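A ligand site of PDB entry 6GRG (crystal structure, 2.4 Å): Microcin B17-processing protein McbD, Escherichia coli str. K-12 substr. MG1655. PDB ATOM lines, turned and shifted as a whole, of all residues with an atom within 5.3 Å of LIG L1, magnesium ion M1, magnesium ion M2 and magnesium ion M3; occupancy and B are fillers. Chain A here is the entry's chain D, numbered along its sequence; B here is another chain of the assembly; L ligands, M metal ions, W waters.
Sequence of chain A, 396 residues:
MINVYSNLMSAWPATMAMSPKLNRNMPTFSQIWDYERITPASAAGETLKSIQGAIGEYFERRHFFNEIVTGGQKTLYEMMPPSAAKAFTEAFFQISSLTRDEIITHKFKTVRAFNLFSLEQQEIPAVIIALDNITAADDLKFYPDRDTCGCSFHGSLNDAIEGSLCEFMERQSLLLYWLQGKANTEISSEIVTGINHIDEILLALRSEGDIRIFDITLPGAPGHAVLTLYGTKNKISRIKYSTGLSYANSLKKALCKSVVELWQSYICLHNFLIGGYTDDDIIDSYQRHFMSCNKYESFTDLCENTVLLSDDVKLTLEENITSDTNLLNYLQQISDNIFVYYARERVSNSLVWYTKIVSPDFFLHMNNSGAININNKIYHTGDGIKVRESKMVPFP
Within 4 Å of magnesium ion M3: Glu 57.
Magnesium ion M1 is bound by water W12 (2.1 Å), OE2 of Glu 261 (2.2 Å), water W5 (2.2 Å), O1 of LG2 L2 (2.2 Å), O1 of LIG L1 (2.2 Å) and water W10 (2.2 Å).
Glu 60 touches magnesium ion M2 (OE1 to MG, 3.8 Å).
Arg 61 touches magnesium ion M2 (NH2 to MG, 3.8 Å).
O of Cys 151 touches magnesium ion M2, 3.7 Å away.
Within 4 Å of magnesium ion M2: Glu 60, Arg 61, Cys 151 and Glu 167.
Along chain A the residues within 4 Å of magnesium ion M2 span positions 60 to 167.
Magnesium ion M2 is bound by O2 of LIG L1, OE1 of Glu 167, water W9, water W7, water W4 and O4 of LG2 L2.
Magnesium ion M2 has six donor atoms within binding distance.
Glu 170 touches magnesium ion M1.
NH2 of Arg 171 touches magnesium ion M1, 3.95 Å away.
Leu 245 touches magnesium ion M1 (O to MG, 3.8 Å).
Lys 257 touches magnesium ion M1.
Water W5 lies within hydrogen-bond range of the backbone carbonyl oxygen of Leu 245 (2.5 Å), the side-chain amino group of Lys 257 (2.9 Å) and the side-chain carboxylate of Glu 261 (3.4 Å).
Water W12 bridges OE1 of Glu 170 (2.6 Å) and NH2 of Arg 171 (3.4 Å).
Water W9 bridges OE1 of Glu 60 (2.9 Å) and NH2 of Arg 61 (3.1 Å).
Water W1 lies within hydrogen-bond range of O5 of LIG L1 (2.5 Å), O of Ser 42 (2.7 Å) and OE1 of Gln 264 (3.3 Å).
Water W8 lies within hydrogen-bond range of a nitrogen (N4) of LIG L1, the backbone carbonyl oxygen (O) of Leu 222 of chain B, the backbone NH (N) of Gly 155 and a ring nitrogen (ND1) of His 154.
Water W3 bridges O5 of LIG L1 (2.7 Å) and N of Ala 44 (2.9 Å).
Water W6 is bound to magnesium ion M3 (2.1 Å).
O3 of LIG L1 is bound to magnesium ion M3 (2.1 Å).
Magnesium ion M3 is bound by water W11, 2.1 Å away.
Magnesium ion M3 is bound by the side-chain carboxylate (OE1) of Glu 57, at 2.2 Å.
O3 of LG2 L2 is bound to magnesium ion M3 (2.2 Å).
Magnesium ion M3 is bound by water W1 (2.2 Å).
The backbone NH of Glu 57 is in hydrogen-bond range of an oxygen (O8) of LIG L1 (3.4 Å).
The side-chain carboxylate of Glu 60 is in hydrogen-bond range of an oxygen (O9) of LIG L1, at 2.8 Å.
The backbone carbonyl oxygen (O) of Leu 222 of chain B is in hydrogen-bond range of a nitrogen (N3) of LIG L1.
O9 of LIG L1 sits at hydrogen-bond distance from N of Phe 153, 3.0 Å away.
O1 of LIG L1 lies close to NZ of Lys 257 (2.9 Å).
O10 of LIG L1 sits at hydrogen-bond distance from O of Phe 153 (2.5 Å).
O of Gly 53 lies close to O8 of LIG L1, 3.1 Å away.
Ala 43 touches LIG L1.
Gln 52 touches LIG L1 (CD to N3, 3.5 Å).
Gly 56 touches LIG L1.
Ser 152 touches LIG L1 (CA to O9, 3.9 Å).
His 154 touches LIG L1 (NE2 to C7, 3.3 Å).
Hydrophobic or aromatic side chains that line LIG L1: Ala 43, Phe 153, His 154 and Leu 222 of chain B.
Of the 24 residues printed, 13 come within 4 Å of LIG L1.
The nearest printed residue that does not touch LIG L1 is Gly 155 (4.1 Å).
O of Leu 222 of chain B is in hydrogen-bond range of NE2 of Gln 52, 3.3 Å away.
OE1 of Glu 261 is in hydrogen-bond range of N of Leu 245 (3.3 Å).
The backbone NH (N) of Ser 42 lies within hydrogen-bond range of the side-chain carboxylate (OE2) of Glu 57, 3.1 Å away.
The side-chain carboxylate (OE2) of Glu 60 lies within salt-bridge range of the guanidinium group (NE) of Arg 61 (2.9 Å).
The guanidinium group of Arg 171 lies close to the side-chain carboxylate of Glu 167 (3.8 Å).
The backbone NH of Cys 151 is in hydrogen-bond range of the side-chain carboxylate of Glu 167 (3.5 Å).
The guanidinium group of Arg 171 is in salt-bridge range of the side-chain carboxylate of Glu 170, at 3.1 Å.
The side-chain carboxylate (OE2) of Glu 261 sits close to the side-chain amino group (NZ) of Lys 257.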
ATOM      1  N   SER A  42       7.715  33.287 -21.368  1.00  0.00           N
ATOM      2  CA  SER A  42       7.102  34.585 -21.319  1.00  0.00           C
ATOM      3  C   SER A  42       5.762  34.574 -22.083  1.00  0.00           C
ATOM      4  O   SER A  42       5.454  33.652 -22.876  1.00  0.00           O
ATOM      5  CB  SER A  42       8.027  35.644 -21.876  1.00  0.00           C
ATOM      6  OG  SER A  42       7.876  35.756 -23.281  1.00  0.00           O
ATOM      7  N   ALA A  43       4.983  35.631 -21.839  1.00  0.00           N
ATOM      8  CA  ALA A  43       3.725  35.851 -22.535  1.00  0.00           C
ATOM      9  C   ALA A  43       3.444  37.347 -22.518  1.00  0.00           C
ATOM     10  O   ALA A  43       4.070  38.078 -21.760  1.00  0.00           O
ATOM     11  CB  ALA A  43       2.623  35.018 -21.904  1.00  0.00           C
ATOM     12  N   ALA A  44       2.529  37.793 -23.385  1.00  0.00           N
ATOM     13  CA  ALA A  44       2.221  39.203 -23.473  1.00  0.00           C
ATOM     14  C   ALA A  44       0.759  39.399 -23.884  1.00  0.00           C
ATOM     15  O   ALA A  44       0.186  38.529 -24.540  1.00  0.00           O
ATOM     16  CB  ALA A  44       3.191  39.855 -24.442  1.00  0.00           C
ATOM     17  N   LYS A  49      -3.857  37.676 -18.694  1.00  0.00           N
ATOM     18  CA  LYS A  49      -3.554  36.794 -19.833  1.00  0.00           C
ATOM     19  C   LYS A  49      -2.031  36.588 -19.885  1.00  0.00           C
ATOM     20  O   LYS A  49      -1.579  35.489 -19.950  1.00  0.00           O
ATOM     21  CB  LYS A  49      -4.066  37.358 -21.163  1.00  0.00           C
ATOM     22  CG  LYS A  49      -5.529  37.058 -21.534  1.00  0.00           C
ATOM     23  N   GLN A  52      -0.940  34.422 -16.964  1.00  0.00           N
ATOM     24  CA  GLN A  52      -1.418  33.037 -17.164  1.00  0.00           C
ATOM     25  C   GLN A  52      -0.540  32.362 -18.238  1.00  0.00           C
ATOM     26  O   GLN A  52      -0.161  31.174 -18.086  1.00  0.00           O
ATOM     27  CB  GLN A  52      -2.900  33.041 -17.553  1.00  0.00           C
ATOM     28  CG  GLN A  52      -3.828  33.373 -16.402  1.00  0.00           C
ATOM     29  CD  GLN A  52      -5.272  33.499 -16.839  1.00  0.00           C
ATOM     30  OE1 GLN A  52      -5.550  34.008 -17.920  1.00  0.00           O
ATOM     31  NE2 GLN A  52      -6.232  33.068 -16.014  1.00  0.00           N
ATOM     32  N   GLY A  53      -0.217  33.122 -19.288  1.00  0.00           N
ATOM     33  CA  GLY A  53       0.545  32.705 -20.456  1.00  0.00           C
ATOM     34  C   GLY A  53       1.985  32.367 -20.125  1.00  0.00           C
ATOM     35  O   GLY A  53       2.501  31.377 -20.608  1.00  0.00           O
ATOM     36  N   ALA A  54       2.640  33.197 -19.303  1.00  0.00           N
ATOM     37  CA  ALA A  54       4.008  32.941 -18.877  1.00  0.00           C
ATOM     38  C   ALA A  54       4.055  31.722 -17.948  1.00  0.00           C
ATOM     39  O   ALA A  54       4.984  30.912 -18.064  1.00  0.00           O
ATOM     40  CB  ALA A  54       4.603  34.152 -18.199  1.00  0.00           C
ATOM     41  N   GLY A  56       1.818  29.266 -17.929  1.00  0.00           N
ATOM     42  CA  GLY A  56       1.482  28.222 -18.863  1.00  0.00           C
ATOM     43  C   GLY A  56       2.658  27.821 -19.750  1.00  0.00           C
ATOM     44  O   GLY A  56       2.935  26.658 -19.942  1.00  0.00           O
ATOM     45  N   GLU A  57       3.378  28.808 -20.280  1.00  0.00           N
ATOM     46  CA  GLU A  57       4.457  28.481 -21.179  1.00  0.00           C
ATOM     47  C   GLU A  57       5.553  27.822 -20.337  1.00  0.00           C
ATOM     48  O   GLU A  57       6.190  26.881 -20.805  1.00  0.00           O
ATOM     49  CB  GLU A  57       4.973  29.715 -21.923  1.00  0.00           C
ATOM     50  CG  GLU A  57       5.891  29.346 -23.078  1.00  0.00           C
ATOM     51  CD  GLU A  57       6.248  30.518 -23.974  1.00  0.00           C
ATOM     52  OE1 GLU A  57       5.539  30.754 -24.992  1.00  0.00           O
ATOM     53  OE2 GLU A  57       7.234  31.187 -23.639  1.00  0.00           O
ATOM     54  N   GLU A  60       4.557  24.163 -19.773  1.00  0.00           N
ATOM     55  CA  GLU A  60       4.680  23.564 -21.084  1.00  0.00           C
ATOM     56  C   GLU A  60       6.130  23.158 -21.367  1.00  0.00           C
ATOM     57  O   GLU A  60       6.421  22.003 -21.622  1.00  0.00           O
ATOM     58  CB  GLU A  60       4.210  24.567 -22.138  1.00  0.00           C
ATOM     59  CG  GLU A  60       4.097  24.023 -23.543  1.00  0.00           C
ATOM     60  CD  GLU A  60       4.093  25.130 -24.581  1.00  0.00           C
ATOM     61  OE1 GLU A  60       3.324  26.096 -24.407  1.00  0.00           O
ATOM     62  OE2 GLU A  60       4.857  25.002 -25.565  1.00  0.00           O
ATOM     63  N   ARG A  61       7.023  24.150 -21.353  1.00  0.00           N
ATOM     64  CA  ARG A  61       8.392  23.981 -21.835  1.00  0.00           C
ATOM     65  C   ARG A  61       9.163  23.069 -20.888  1.00  0.00           C
ATOM     66  O   ARG A  61       9.965  22.240 -21.339  1.00  0.00           O
ATOM     67  CB  ARG A  61       9.040  25.353 -22.020  1.00  0.00           C
ATOM     68  CG  ARG A  61       8.339  26.213 -23.062  1.00  0.00           C
ATOM     69  CD  ARG A  61       8.580  25.754 -24.500  1.00  0.00           C
ATOM     70  NE  ARG A  61       7.539  26.174 -25.444  1.00  0.00           N
ATOM     71  CZ  ARG A  61       7.575  27.303 -26.154  1.00  0.00           C
ATOM     72  NH1 ARG A  61       8.638  28.076 -26.078  1.00  0.00           N
ATOM     73  NH2 ARG A  61       6.550  27.653 -26.928  1.00  0.00           N
ATOM     74  N   CYS A 151       2.972  22.057 -29.169  1.00  0.00           N
ATOM     75  CA  CYS A 151       3.030  21.885 -27.724  1.00  0.00           C
ATOM     76  C   CYS A 151       2.127  22.914 -27.041  1.00  0.00           C
ATOM     77  O   CYS A 151       2.018  24.071 -27.491  1.00  0.00           O
ATOM     78  CB  CYS A 151       4.434  22.068 -27.186  1.00  0.00           C
ATOM     79  SG  CYS A 151       5.578  20.715 -27.604  1.00  0.00           S
ATOM     80  N   SER A 152       1.511  22.495 -25.929  1.00  0.00           N
ATOM     81  CA  SER A 152       0.567  23.353 -25.260  1.00  0.00           C
ATOM     82  C   SER A 152       0.290  22.862 -23.828  1.00  0.00           C
ATOM     83  O   SER A 152       0.389  21.669 -23.537  1.00  0.00           O
ATOM     84  CB  SER A 152      -0.649  23.490 -26.155  1.00  0.00           C
ATOM     85  OG  SER A 152      -1.829  23.587 -25.412  1.00  0.00           O
ATOM     86  N   PHE A 153      -0.003  23.816 -22.919  1.00  0.00           N
ATOM     87  CA  PHE A 153      -0.373  23.555 -21.509  1.00  0.00           C
ATOM     88  C   PHE A 153      -1.683  24.286 -21.182  1.00  0.00           C
ATOM     89  O   PHE A 153      -1.877  25.397 -21.626  1.00  0.00           O
ATOM     90  CB  PHE A 153       0.724  24.036 -20.547  1.00  0.00           C
ATOM     91  CG  PHE A 153       0.390  24.024 -19.071  1.00  0.00           C
ATOM     92  CD1 PHE A 153       0.632  22.892 -18.290  1.00  0.00           C
ATOM     93  CD2 PHE A 153      -0.138  25.139 -18.439  1.00  0.00           C
ATOM     94  CE1 PHE A 153       0.335  22.875 -16.935  1.00  0.00           C
ATOM     95  CE2 PHE A 153      -0.441  25.122 -17.091  1.00  0.00           C
ATOM     96  CZ  PHE A 153      -0.207  23.997 -16.331  1.00  0.00           C
ATOM     97  N   HIS A 154      -2.563  23.645 -20.403  1.00  0.00           N
ATOM     98  CA  HIS A 154      -3.752  24.323 -19.864  1.00  0.00           C
ATOM     99  C   HIS A 154      -4.330  23.495 -18.705  1.00  0.00           C
ATOM    100  O   HIS A 154      -3.896  22.366 -18.483  1.00  0.00           O
ATOM    101  CB  HIS A 154      -4.775  24.561 -20.998  1.00  0.00           C
ATOM    102  CG  HIS A 154      -5.375  25.930 -20.975  1.00  0.00           C
ATOM    103  ND1 HIS A 154      -6.343  26.312 -20.038  1.00  0.00           N
ATOM    104  CD2 HIS A 154      -5.157  27.004 -21.767  1.00  0.00           C
ATOM    105  CE1 HIS A 154      -6.689  27.558 -20.258  1.00  0.00           C
ATOM    106  NE2 HIS A 154      -5.960  28.016 -21.308  1.00  0.00           N
ATOM    107  N   GLY A 155      -5.317  24.082 -17.992  1.00  0.00           N
ATOM    108  CA  GLY A 155      -5.997  23.477 -16.835  1.00  0.00           C
ATOM    109  C   GLY A 155      -7.267  22.725 -17.207  1.00  0.00           C
ATOM    110  O   GLY A 155      -7.857  22.054 -16.367  1.00  0.00           O
ATOM    111  N   GLU A 167      -1.838  25.955 -32.781  1.00  0.00           N
ATOM    112  CA  GLU A 167      -0.393  26.108 -33.052  1.00  0.00           C
ATOM    113  C   GLU A 167       0.032  25.181 -34.212  1.00  0.00           C
ATOM    114  O   GLU A 167       0.725  25.602 -35.142  1.00  0.00           O
ATOM    115  CB  GLU A 167       0.416  25.846 -31.780  1.00  0.00           C
ATOM    116  CG  GLU A 167       1.861  26.225 -31.928  1.00  0.00           C
ATOM    117  CD  GLU A 167       2.665  26.254 -30.634  1.00  0.00           C
ATOM    118  OE1 GLU A 167       2.527  27.250 -29.879  1.00  0.00           O
ATOM    119  OE2 GLU A 167       3.401  25.271 -30.380  1.00  0.00           O
ATOM    120  N   GLU A 170      -0.975  26.764 -37.340  1.00  0.00           N
ATOM    121  CA  GLU A 170      -0.290  28.004 -37.654  1.00  0.00           C
ATOM    122  C   GLU A 170       1.081  27.645 -38.223  1.00  0.00           C
ATOM    123  O   GLU A 170       1.561  28.298 -39.153  1.00  0.00           O
ATOM    124  CB  GLU A 170      -0.301  28.954 -36.446  1.00  0.00           C
ATOM    125  CG  GLU A 170       0.925  28.839 -35.571  1.00  0.00           C
ATOM    126  CD  GLU A 170       0.944  29.557 -34.238  1.00  0.00           C
ATOM    127  OE1 GLU A 170       2.056  29.828 -33.761  1.00  0.00           O
ATOM    128  OE2 GLU A 170      -0.157  29.835 -33.668  1.00  0.00           O
ATOM    129  N   ARG A 171       1.709  26.600 -37.659  1.00  0.00           N
ATOM    130  CA  ARG A 171       3.047  26.232 -38.033  1.00  0.00           C
ATOM    131  C   ARG A 171       3.004  25.435 -39.344  1.00  0.00           C
ATOM    132  O   ARG A 171       3.929  25.568 -40.183  1.00  0.00           O
ATOM    133  CB  ARG A 171       3.727  25.534 -36.862  1.00  0.00           C
ATOM    134  CG  ARG A 171       3.804  26.396 -35.606  1.00  0.00           C
ATOM    135  CD  ARG A 171       4.678  27.636 -35.791  1.00  0.00           C
ATOM    136  NE  ARG A 171       4.759  28.449 -34.589  1.00  0.00           N
ATOM    137  CZ  ARG A 171       5.293  28.028 -33.448  1.00  0.00           C
ATOM    138  NH1 ARG A 171       5.996  26.903 -33.421  1.00  0.00           N
ATOM    139  NH2 ARG A 171       5.066  28.708 -32.327  1.00  0.00           N
ATOM    140  N   LEU A 245       2.816  35.420 -35.199  1.00  0.00           N
ATOM    141  CA  LEU A 245       1.928  34.472 -35.852  1.00  0.00           C
ATOM    142  C   LEU A 245       0.967  33.863 -34.826  1.00  0.00           C
ATOM    143  O   LEU A 245       1.345  33.507 -33.716  1.00  0.00           O
ATOM    144  CB  LEU A 245       2.775  33.399 -36.540  1.00  0.00           C
ATOM    145  CG  LEU A 245       2.038  32.174 -37.114  1.00  0.00           C
ATOM    146  CD1 LEU A 245       1.051  32.555 -38.218  1.00  0.00           C
ATOM    147  CD2 LEU A 245       3.033  31.163 -37.640  1.00  0.00           C
ATOM    148  N   LYS A 257      -3.330  38.401 -31.431  1.00  0.00           N
ATOM    149  CA  LYS A 257      -2.270  37.572 -30.865  1.00  0.00           C
ATOM    150  C   LYS A 257      -1.010  37.663 -31.744  1.00  0.00           C
ATOM    151  O   LYS A 257       0.151  37.759 -31.250  1.00  0.00           O
ATOM    152  CB  LYS A 257      -2.778  36.128 -30.702  1.00  0.00           C
ATOM    153  CG  LYS A 257      -1.746  35.122 -30.212  1.00  0.00           C
ATOM    154  CD  LYS A 257      -1.223  35.414 -28.812  1.00  0.00           C
ATOM    155  CE  LYS A 257      -0.235  34.364 -28.310  1.00  0.00           C
ATOM    156  NZ  LYS A 257       1.111  34.513 -28.926  1.00  0.00           N
ATOM    157  N   GLU A 261       2.518  38.971 -30.329  1.00  0.00           N
ATOM    158  CA  GLU A 261       3.657  38.084 -30.395  1.00  0.00           C
ATOM    159  C   GLU A 261       4.807  38.785 -31.164  1.00  0.00           C
ATOM    160  O   GLU A 261       5.951  38.675 -30.779  1.00  0.00           O
ATOM    161  CB  GLU A 261       3.248  36.725 -30.989  1.00  0.00           C
ATOM    162  CG  GLU A 261       4.312  35.650 -30.820  1.00  0.00           C
ATOM    163  CD  GLU A 261       3.935  34.234 -31.244  1.00  0.00           C
ATOM    164  OE1 GLU A 261       4.017  33.938 -32.465  1.00  0.00           O
ATOM    165  OE2 GLU A 261       3.557  33.423 -30.366  1.00  0.00           O
ATOM    166  N   GLN A 264       6.299  40.961 -28.715  1.00  0.00           N
ATOM    167  CA  GLN A 264       6.905  40.112 -27.699  1.00  0.00           C
ATOM    168  C   GLN A 264       8.332  39.720 -28.145  1.00  0.00           C
ATOM    169  O   GLN A 264       9.284  39.848 -27.390  1.00  0.00           O
ATOM    170  CB  GLN A 264       6.008  38.899 -27.407  1.00  0.00           C
ATOM    171  CG  GLN A 264       6.596  37.922 -26.397  1.00  0.00           C
ATOM    172  CD  GLN A 264       5.925  36.571 -26.362  1.00  0.00           C
ATOM    173  OE1 GLN A 264       6.224  35.738 -25.496  1.00  0.00           O
ATOM    174  NE2 GLN A 264       4.995  36.352 -27.262  1.00  0.00           N
ATOM    175  N   LEU B 222      -4.483  30.750 -12.735  1.00  0.00           N
ATOM    176  CA  LEU B 222      -4.667  30.039 -14.024  1.00  0.00           C
ATOM    177  C   LEU B 222      -6.149  29.781 -14.327  1.00  0.00           C
ATOM    178  O   LEU B 222      -6.529  29.798 -15.504  1.00  0.00           O
ATOM    179  CB  LEU B 222      -3.915  28.712 -14.005  1.00  0.00           C
ATOM    180  CG  LEU B 222      -2.400  28.851 -13.879  1.00  0.00           C
ATOM    181  CD1 LEU B 222      -1.742  27.484 -13.898  1.00  0.00           C
ATOM    182  CD2 LEU B 222      -1.843  29.749 -14.970  1.00  0.00           C
HETATM  183  P1  LIG L   1       1.899  30.896 -27.548  1.00  0.00           P
HETATM  184  O1  LIG L   1       2.071  31.771 -28.763  1.00  0.00           O
HETATM  185  O2  LIG L   1       1.520  29.445 -27.763  1.00  0.00           O
HETATM  186  O3  LIG L   1       2.993  30.966 -26.545  1.00  0.00           O
HETATM  187  P2  LIG L   1       0.272  32.067 -25.385  1.00  0.00           P
HETATM  188  O4  LIG L   1      -1.175  32.482 -25.531  1.00  0.00           O
HETATM  189  O5  LIG L   1       1.383  33.024 -25.017  1.00  0.00           O
HETATM  190  O6  LIG L   1       0.538  31.475 -26.878  1.00  0.00           O
HETATM  191  O7  LIG L   1       0.297  30.826 -24.385  1.00  0.00           O
HETATM  192  C1  LIG L   1       1.510  30.357 -23.812  1.00  0.00           C
HETATM  193  C2  LIG L   1       1.231  29.083 -23.016  1.00  0.00           C
HETATM  194  O8  LIG L   1       0.431  29.407 -21.866  1.00  0.00           O
HETATM  195  C3  LIG L   1       0.439  28.020 -23.770  1.00  0.00           C
HETATM  196  O9  LIG L   1       0.832  26.690 -23.341  1.00  0.00           O
HETATM  197  C4  LIG L   1      -0.967  28.250 -23.297  1.00  0.00           C
HETATM  198  O10 LIG L   1      -1.798  27.098 -23.435  1.00  0.00           O
HETATM  199  C5  LIG L   1      -0.720  28.574 -21.829  1.00  0.00           C
HETATM  200  N1  LIG L   1      -1.860  29.239 -21.187  1.00  0.00           N
HETATM  201  C6  LIG L   1      -2.452  30.377 -21.602  1.00  0.00           C
HETATM  202  N2  LIG L   1      -3.480  30.714 -20.784  1.00  0.00           N
HETATM  203  C7  LIG L   1      -3.557  29.773 -19.813  1.00  0.00           C
HETATM  204  C8  LIG L   1      -4.407  29.536 -18.631  1.00  0.00           C
HETATM  205  N3  LIG L   1      -5.399  30.371 -18.322  1.00  0.00           N
HETATM  206  N4  LIG L   1      -4.168  28.439 -17.863  1.00  0.00           N
HETATM  207  C9  LIG L   1      -3.158  27.590 -18.173  1.00  0.00           C
HETATM  208  N5  LIG L   1      -2.337  27.755 -19.238  1.00  0.00           N
HETATM  209  C10 LIG L   1      -2.488  28.806 -20.090  1.00  0.00           C
HETATM  210  P1  LG2 L   2       5.335  29.996 -29.030  1.00  0.00           P
HETATM  211  O1  LG2 L   2       4.537  31.006 -29.803  1.00  0.00           O
HETATM  212  O2  LG2 L   2       6.571  29.660 -29.851  1.00  0.00           O
HETATM  213  O3  LG2 L   2       5.821  30.591 -27.713  1.00  0.00           O
HETATM  214  O4  LG2 L   2       4.504  28.750 -28.738  1.00  0.00           O
HETATM  215 MG    MG M   1       2.688  31.492 -30.837  1.00  0.00          MG
HETATM  216 MG    MG M   2       2.825  27.715 -27.784  1.00  0.00          MG
HETATM  217 MG    MG M   3       4.795  32.116 -26.518  1.00  0.00          MG
HETATM  218  O   HOH W   1       3.890  33.446 -25.028  1.00  0.00           O
HETATM  219  O   HOH W   2      -0.960  27.750 -27.788  1.00  0.00           O
HETATM  220  O   HOH W   3       1.492  35.690 -25.097  1.00  0.00           O
HETATM  221  O   HOH W   4       1.060  26.550 -27.208  1.00  0.00           O
HETATM  222  O   HOH W   5       1.056  32.842 -31.326  1.00  0.00           O
HETATM  223  O   HOH W   6       6.665  32.891 -25.836  1.00  0.00           O
HETATM  224  O   HOH W   7       4.320  26.142 -27.953  1.00  0.00           O
HETATM  225  O   HOH W   8      -5.990  26.958 -16.661  1.00  0.00           O
HETATM  226  O   HOH W   9       3.722  28.489 -25.969  1.00  0.00           O
HETATM  227  O   HOH W  10       3.647  31.532 -32.801  1.00  0.00           O
HETATM  228  O   HOH W  11       4.848  33.751 -27.904  1.00  0.00           O
HETATM  229  O   HOH W  12       1.951  29.517 -31.183  1.00  0.00           O
